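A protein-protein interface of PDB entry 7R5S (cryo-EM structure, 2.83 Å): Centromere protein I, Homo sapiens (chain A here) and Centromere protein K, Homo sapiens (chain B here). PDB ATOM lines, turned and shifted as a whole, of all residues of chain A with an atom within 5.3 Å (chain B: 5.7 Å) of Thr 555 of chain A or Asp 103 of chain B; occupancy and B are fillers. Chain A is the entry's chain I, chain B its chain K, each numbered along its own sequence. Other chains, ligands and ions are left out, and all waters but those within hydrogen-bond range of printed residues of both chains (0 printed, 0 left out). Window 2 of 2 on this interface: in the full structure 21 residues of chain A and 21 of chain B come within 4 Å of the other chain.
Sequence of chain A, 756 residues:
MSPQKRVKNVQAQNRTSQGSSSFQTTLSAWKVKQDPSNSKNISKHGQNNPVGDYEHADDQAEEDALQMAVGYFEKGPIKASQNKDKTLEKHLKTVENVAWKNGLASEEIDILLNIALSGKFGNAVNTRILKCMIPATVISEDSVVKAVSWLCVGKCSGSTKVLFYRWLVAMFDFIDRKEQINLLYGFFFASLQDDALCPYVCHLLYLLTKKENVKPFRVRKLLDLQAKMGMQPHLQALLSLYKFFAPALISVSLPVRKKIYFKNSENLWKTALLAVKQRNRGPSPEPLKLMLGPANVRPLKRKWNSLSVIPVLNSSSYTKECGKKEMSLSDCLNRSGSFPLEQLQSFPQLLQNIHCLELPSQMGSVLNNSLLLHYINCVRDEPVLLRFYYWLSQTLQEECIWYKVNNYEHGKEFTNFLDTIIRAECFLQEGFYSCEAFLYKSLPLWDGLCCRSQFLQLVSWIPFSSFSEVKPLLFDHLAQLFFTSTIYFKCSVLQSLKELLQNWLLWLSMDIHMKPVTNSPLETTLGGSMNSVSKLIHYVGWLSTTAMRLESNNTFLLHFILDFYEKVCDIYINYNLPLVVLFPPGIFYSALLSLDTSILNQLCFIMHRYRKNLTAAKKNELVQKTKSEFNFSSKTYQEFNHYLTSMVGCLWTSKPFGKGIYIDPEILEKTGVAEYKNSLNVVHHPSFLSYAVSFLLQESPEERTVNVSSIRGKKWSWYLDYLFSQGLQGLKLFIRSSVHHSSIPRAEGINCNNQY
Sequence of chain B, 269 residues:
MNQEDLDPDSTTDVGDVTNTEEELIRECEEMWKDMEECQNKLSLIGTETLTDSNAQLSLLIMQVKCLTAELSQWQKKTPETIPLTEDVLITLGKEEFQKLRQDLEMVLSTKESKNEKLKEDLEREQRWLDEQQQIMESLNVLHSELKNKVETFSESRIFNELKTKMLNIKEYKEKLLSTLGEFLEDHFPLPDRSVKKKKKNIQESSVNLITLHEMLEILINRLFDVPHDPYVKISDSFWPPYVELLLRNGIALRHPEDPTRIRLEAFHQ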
ATOM      1  N   ASN A 553       4.293  -6.807   1.805  1.00  0.00           N
ATOM      2  CA  ASN A 553       3.674  -6.375   3.059  1.00  0.00           C
ATOM      3  C   ASN A 553       4.452  -5.226   3.706  1.00  0.00           C
ATOM      4  O   ASN A 553       5.001  -5.347   4.803  1.00  0.00           O
ATOM      5  CB  ASN A 553       3.526  -7.553   4.028  1.00  0.00           C
ATOM      6  CG  ASN A 553       2.572  -8.612   3.515  1.00  0.00           C
ATOM      7  OD1 ASN A 553       1.590  -8.305   2.841  1.00  0.00           O
ATOM      8  ND2 ASN A 553       2.857  -9.869   3.833  1.00  0.00           N
ATOM      9  N   ASN A 554       4.489  -4.097   3.002  1.00  0.00           N
ATOM     10  CA  ASN A 554       5.116  -2.888   3.518  1.00  0.00           C
ATOM     11  C   ASN A 554       4.075  -2.055   4.257  1.00  0.00           C
ATOM     12  O   ASN A 554       2.973  -1.830   3.746  1.00  0.00           O
ATOM     13  CB  ASN A 554       5.742  -2.078   2.383  1.00  0.00           C
ATOM     14  CG  ASN A 554       6.811  -1.119   2.871  1.00  0.00           C
ATOM     15  OD1 ASN A 554       6.795  -0.685   4.021  1.00  0.00           O
ATOM     16  ND2 ASN A 554       7.750  -0.787   1.994  1.00  0.00           N
ATOM     17  N   THR A 555       4.430  -1.596   5.460  1.00  0.00           N
ATOM     18  CA  THR A 555       3.481  -0.835   6.267  1.00  0.00           C
ATOM     19  C   THR A 555       3.271   0.572   5.720  1.00  0.00           C
ATOM     20  O   THR A 555       2.222   1.181   5.968  1.00  0.00           O
ATOM     21  CB  THR A 555       3.957  -0.773   7.720  1.00  0.00           C
ATOM     22  OG1 THR A 555       3.139   0.146   8.456  1.00  0.00           O
ATOM     23  CG2 THR A 555       5.406  -0.322   7.787  1.00  0.00           C
ATOM     24  N   PHE A 556       4.248   1.100   4.980  1.00  0.00           N
ATOM     25  CA  PHE A 556       4.111   2.435   4.408  1.00  0.00           C
ATOM     26  C   PHE A 556       2.942   2.511   3.435  1.00  0.00           C
ATOM     27  O   PHE A 556       2.330   3.574   3.282  1.00  0.00           O
ATOM     28  CB  PHE A 556       5.414   2.840   3.715  1.00  0.00           C
ATOM     29  CG  PHE A 556       5.471   4.289   3.327  1.00  0.00           C
ATOM     30  CD1 PHE A 556       5.674   5.268   4.283  1.00  0.00           C
ATOM     31  CD2 PHE A 556       5.328   4.672   2.004  1.00  0.00           C
ATOM     32  CE1 PHE A 556       5.730   6.602   3.930  1.00  0.00           C
ATOM     33  CE2 PHE A 556       5.382   6.004   1.643  1.00  0.00           C
ATOM     34  CZ  PHE A 556       5.583   6.971   2.608  1.00  0.00           C
ATOM     35  N   LEU A 557       2.615   1.401   2.775  1.00  0.00           N
ATOM     36  CA  LEU A 557       1.454   1.335   1.895  1.00  0.00           C
ATOM     37  C   LEU A 557       0.175   0.996   2.648  1.00  0.00           C
ATOM     38  O   LEU A 557      -0.903   1.497   2.292  1.00  0.00           O
ATOM     39  CB  LEU A 557       1.698   0.299   0.795  1.00  0.00           C
ATOM     40  CG  LEU A 557       0.680   0.211  -0.342  1.00  0.00           C
ATOM     41  CD1 LEU A 557       0.737   1.457  -1.208  1.00  0.00           C
ATOM     42  CD2 LEU A 557       0.936  -1.034  -1.169  1.00  0.00           C
ATOM     43  N   LEU A 558       0.275   0.154   3.679  1.00  0.00           N
ATOM     44  CA  LEU A 558      -0.888  -0.160   4.498  1.00  0.00           C
ATOM     45  C   LEU A 558      -1.426   1.082   5.193  1.00  0.00           C
ATOM     46  O   LEU A 558      -2.637   1.190   5.421  1.00  0.00           O
ATOM     47  CB  LEU A 558      -0.530  -1.237   5.523  1.00  0.00           C
ATOM     48  CG  LEU A 558      -1.683  -1.856   6.313  1.00  0.00           C
ATOM     49  CD1 LEU A 558      -2.678  -2.520   5.376  1.00  0.00           C
ATOM     50  CD2 LEU A 558      -1.155  -2.853   7.331  1.00  0.00           C
ATOM     51  N   HIS A 559      -0.549   2.033   5.524  1.00  0.00           N
ATOM     52  CA  HIS A 559      -1.012   3.290   6.103  1.00  0.00           C
ATOM     53  C   HIS A 559      -1.936   4.033   5.146  1.00  0.00           C
ATOM     54  O   HIS A 559      -3.007   4.502   5.546  1.00  0.00           O
ATOM     55  CB  HIS A 559       0.181   4.165   6.489  1.00  0.00           C
ATOM     56  CG  HIS A 559       0.662   3.946   7.889  1.00  0.00           C
ATOM     57  ND1 HIS A 559       1.602   2.991   8.214  1.00  0.00           N
ATOM     58  CD2 HIS A 559       0.329   4.556   9.052  1.00  0.00           C
ATOM     59  CE1 HIS A 559       1.829   3.025   9.515  1.00  0.00           C
ATOM     60  NE2 HIS A 559       1.070   3.965  10.046  1.00  0.00           N
ATOM     61  N   PHE A 560      -1.548   4.138   3.872  1.00  0.00           N
ATOM     62  CA  PHE A 560      -2.396   4.814   2.895  1.00  0.00           C
ATOM     63  C   PHE A 560      -3.681   4.033   2.639  1.00  0.00           C
ATOM     64  O   PHE A 560      -4.750   4.628   2.449  1.00  0.00           O
ATOM     65  CB  PHE A 560      -1.628   5.025   1.589  1.00  0.00           C
ATOM     66  CG  PHE A 560      -0.640   6.154   1.644  1.00  0.00           C
ATOM     67  CD1 PHE A 560       0.630   5.956   2.154  1.00  0.00           C
ATOM     68  CD2 PHE A 560      -0.982   7.413   1.180  1.00  0.00           C
ATOM     69  CE1 PHE A 560       1.542   6.993   2.205  1.00  0.00           C
ATOM     70  CE2 PHE A 560      -0.074   8.453   1.227  1.00  0.00           C
ATOM     71  CZ  PHE A 560       1.189   8.243   1.740  1.00  0.00           C
ATOM     72  N   ASP A 596       3.051  -3.099  13.779  1.00  0.00           N
ATOM     73  CA  ASP A 596       2.832  -1.690  14.065  1.00  0.00           C
ATOM     74  C   ASP A 596       1.647  -1.519  15.008  1.00  0.00           C
ATOM     75  O   ASP A 596       0.622  -2.192  14.870  1.00  0.00           O
ATOM     76  CB  ASP A 596       2.586  -0.924  12.765  1.00  0.00           C
ATOM     77  CG  ASP A 596       2.823   0.565  12.905  1.00  0.00           C
ATOM     78  OD1 ASP A 596       2.450   1.144  13.946  1.00  0.00           O
ATOM     79  OD2 ASP A 596       3.378   1.160  11.959  1.00  0.00           O
ATOM     80  N   ILE A 599      -1.178   0.916  13.361  1.00  0.00           N
ATOM     81  CA  ILE A 599      -2.058   0.154  12.479  1.00  0.00           C
ATOM     82  C   ILE A 599      -3.196  -0.471  13.276  1.00  0.00           C
ATOM     83  O   ILE A 599      -4.361  -0.420  12.862  1.00  0.00           O
ATOM     84  CB  ILE A 599      -1.253  -0.908  11.707  1.00  0.00           C
ATOM     85  CG1 ILE A 599      -0.292  -0.239  10.723  1.00  0.00           C
ATOM     86  CG2 ILE A 599      -2.185  -1.860  10.976  1.00  0.00           C
ATOM     87  CD1 ILE A 599      -0.980   0.592   9.664  1.00  0.00           C
ATOM     88  N   LYS B  99      13.563  -2.250  10.579  1.00  0.00           N
ATOM     89  CA  LYS B  99      12.964  -1.604   9.409  1.00  0.00           C
ATOM     90  C   LYS B  99      11.731  -0.787   9.791  1.00  0.00           C
ATOM     91  O   LYS B  99      11.489   0.295   9.228  1.00  0.00           O
ATOM     92  CB  LYS B  99      12.614  -2.647   8.347  1.00  0.00           C
ATOM     93  CG  LYS B  99      13.810  -3.425   7.829  1.00  0.00           C
ATOM     94  CD  LYS B  99      13.464  -4.877   7.552  1.00  0.00           C
ATOM     95  CE  LYS B  99      14.714  -5.686   7.253  1.00  0.00           C
ATOM     96  NZ  LYS B  99      15.747  -5.509   8.309  1.00  0.00           N
ATOM     97  N   LEU B 100      10.940  -1.288  10.746  1.00  0.00           N
ATOM     98  CA  LEU B 100       9.754  -0.567  11.192  1.00  0.00           C
ATOM     99  C   LEU B 100      10.112   0.800  11.756  1.00  0.00           C
ATOM    100  O   LEU B 100       9.304   1.730  11.675  1.00  0.00           O
ATOM    101  CB  LEU B 100       9.003  -1.396  12.237  1.00  0.00           C
ATOM    102  CG  LEU B 100       7.660  -0.856  12.725  1.00  0.00           C
ATOM    103  CD1 LEU B 100       6.650  -0.833  11.590  1.00  0.00           C
ATOM    104  CD2 LEU B 100       7.137  -1.680  13.893  1.00  0.00           C
ATOM    105  N   ARG B 101      11.310   0.940  12.322  1.00  0.00           N
ATOM    106  CA  ARG B 101      11.750   2.242  12.825  1.00  0.00           C
ATOM    107  C   ARG B 101      11.729   3.304  11.723  1.00  0.00           C
ATOM    108  O   ARG B 101      11.075   4.353  11.854  1.00  0.00           O
ATOM    109  CB  ARG B 101      13.148   2.111  13.431  1.00  0.00           C
ATOM    110  CG  ARG B 101      13.728   3.408  13.968  1.00  0.00           C
ATOM    111  CD  ARG B 101      15.088   3.173  14.605  1.00  0.00           C
ATOM    112  NE  ARG B 101      15.716   4.418  15.039  1.00  0.00           N
ATOM    113  CZ  ARG B 101      16.891   4.487  15.657  1.00  0.00           C
ATOM    114  NH1 ARG B 101      17.571   3.380  15.920  1.00  0.00           N
ATOM    115  NH2 ARG B 101      17.385   5.664  16.015  1.00  0.00           N
ATOM    116  N   GLN B 102      12.449   3.053  10.625  1.00  0.00           N
ATOM    117  CA  GLN B 102      12.491   4.023   9.534  1.00  0.00           C
ATOM    118  C   GLN B 102      11.127   4.171   8.872  1.00  0.00           C
ATOM    119  O   GLN B 102      10.750   5.273   8.445  1.00  0.00           O
ATOM    120  CB  GLN B 102      13.545   3.622   8.502  1.00  0.00           C
ATOM    121  CG  GLN B 102      14.951   3.482   9.060  1.00  0.00           C
ATOM    122  CD  GLN B 102      15.445   2.052   9.038  1.00  0.00           C
ATOM    123  OE1 GLN B 102      14.661   1.117   8.893  1.00  0.00           O
ATOM    124  NE2 GLN B 102      16.753   1.873   9.184  1.00  0.00           N
ATOM    125  N   ASP B 103      10.372   3.071   8.771  1.00  0.00           N
ATOM    126  CA  ASP B 103       9.018   3.184   8.237  1.00  0.00           C
ATOM    127  C   ASP B 103       8.187   4.168   9.055  1.00  0.00           C
ATOM    128  O   ASP B 103       7.495   5.032   8.496  1.00  0.00           O
ATOM    129  CB  ASP B 103       8.352   1.809   8.204  1.00  0.00           C
ATOM    130  CG  ASP B 103       9.076   0.835   7.294  1.00  0.00           C
ATOM    131  OD1 ASP B 103       9.748   1.292   6.346  1.00  0.00           O
ATOM    132  OD2 ASP B 103       8.970  -0.387   7.527  1.00  0.00           O
ATOM    133  N   LEU B 104       8.271   4.072  10.384  1.00  0.00           N
ATOM    134  CA  LEU B 104       7.505   4.956  11.253  1.00  0.00           C
ATOM    135  C   LEU B 104       7.973   6.400  11.132  1.00  0.00           C
ATOM    136  O   LEU B 104       7.152   7.324  11.159  1.00  0.00           O
ATOM    137  CB  LEU B 104       7.604   4.482  12.702  1.00  0.00           C
ATOM    138  CG  LEU B 104       6.777   3.250  13.064  1.00  0.00           C
ATOM    139  CD1 LEU B 104       7.003   2.861  14.515  1.00  0.00           C
ATOM    140  CD2 LEU B 104       5.308   3.520  12.804  1.00  0.00           C
ATOM    141  N   GLU B 105       9.284   6.620  11.007  1.00  0.00           N
ATOM    142  CA  GLU B 105       9.754   8.000  10.883  1.00  0.00           C
ATOM    143  C   GLU B 105       9.266   8.634   9.578  1.00  0.00           C
ATOM    144  O   GLU B 105       8.857   9.807   9.560  1.00  0.00           O
ATOM    145  CB  GLU B 105      11.280   8.062  11.007  1.00  0.00           C
ATOM    146  CG  GLU B 105      12.072   7.735   9.754  1.00  0.00           C
ATOM    147  CD  GLU B 105      13.564   7.672  10.008  1.00  0.00           C
ATOM    148  OE1 GLU B 105      13.969   7.735  11.188  1.00  0.00           O
ATOM    149  OE2 GLU B 105      14.333   7.561   9.030  1.00  0.00           O
ATOM    150  N   MET B 106       9.257   7.862   8.485  1.00  0.00           N
ATOM    151  CA  MET B 106       8.731   8.388   7.227  1.00  0.00           C
ATOM    152  C   MET B 106       7.237   8.677   7.332  1.00  0.00           C
ATOM    153  O   MET B 106       6.756   9.711   6.843  1.00  0.00           O
ATOM    154  CB  MET B 106       9.013   7.409   6.088  1.00  0.00           C
ATOM    155  CG  MET B 106      10.492   7.185   5.817  1.00  0.00           C
ATOM    156  SD  MET B 106      10.793   6.048   4.451  1.00  0.00           S
ATOM    157  CE  MET B 106      10.076   6.958   3.088  1.00  0.00           C
ATOM    158  N   VAL B 107       6.487   7.771   7.969  1.00  0.00           N
ATOM    159  CA  VAL B 107       5.056   7.998   8.167  1.00  0.00           C
ATOM    160  C   VAL B 107       4.822   9.277   8.964  1.00  0.00           C
ATOM    161  O   VAL B 107       3.916  10.063   8.655  1.00  0.00           O
ATOM    162  CB  VAL B 107       4.413   6.776   8.849  1.00  0.00           C
ATOM    163  CG1 VAL B 107       2.997   7.096   9.296  1.00  0.00           C
ATOM    164  CG2 VAL B 107       4.417   5.583   7.909  1.00  0.00           C
ATOM    165  N   LEU B 108       5.639   9.508   9.994  1.00  0.00           N
ATOM    166  CA  LEU B 108       5.488  10.705  10.817  1.00  0.00           C
ATOM    167  C   LEU B 108       5.726  11.970  10.001  1.00  0.00           C
ATOM    168  O   LEU B 108       4.969  12.947  10.107  1.00  0.00           O
ATOM    169  CB  LEU B 108       6.448  10.636  12.007  1.00  0.00           C
ATOM    170  CG  LEU B 108       6.625  11.882  12.877  1.00  0.00           C
ATOM    171  CD1 LEU B 108       6.638  11.492  14.341  1.00  0.00           C
ATOM    172  CD2 LEU B 108       7.908  12.615  12.517  1.00  0.00           C
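The side-chain amide oxygen (OD1) of Asn 554 of chain A sits close to the backbone NH (N) of Phe 556 of chain A (3.3 Å).
The backbone carbonyl oxygen of Thr 555 of chain A sits at hydrogen-bond distance from a ring nitrogen (ND1) of His 559 of chain A.
CG2 of Thr 555 of chain A touches OD2 of Asp 103 of chain B (3.6 Å).
Phe 556 of chain A touches Val 107 of chain B.
His 559 of chain A touches Val 107 of chain B.
Asp 596 of chain A touches Leu 100 of chain B (OD2 to CD1, 3.8 Å).
Leu 104 of chain B touches Asp 596 of chain A (CD2 to OD2, 3.2 Å).
Thr 555 of chain A touches just one residue of chain B: Asp 103 (3.6 Å).
Of the printed residues of chain B, Phe 556 of chain A touches Val 107 (3.9 Å).
Of the printed residues of chain B, Asp 596 of chain A touches Leu 100 (3.8 Å) and Leu 104 (3.2 Å).
Ile 599 of chain A touches none of the printed residues of chain B.
Of the printed residues of chain A, Leu 100 of chain B touches Asp 596 (3.8 Å).
Gln 102 of chain B touches none of the printed residues of chain A.
Asp 103 of chain B touches one residue of chain A.
Of the printed residues of chain A, Leu 104 of chain B touches Asp 596.
Of the 10 printed residues of chain B, 4 touch a printed residue of chain A.
Hydrophobic or aromatic side chains of chain B that line the printed part of chain A: Leu 100, Leu 104 and Val 107.
Of the 10 printed residues of chain A, 4 touch a printed residue of chain B.
Hydrophobic or aromatic side chains of chain A within 4 Å of the printed part of chain B: Phe 556 and His 559.
Among the printed residues, no Asp or Glu carboxylate lies within 4 Å of a Lys or Arg side-chain nitrogen of the other chain.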
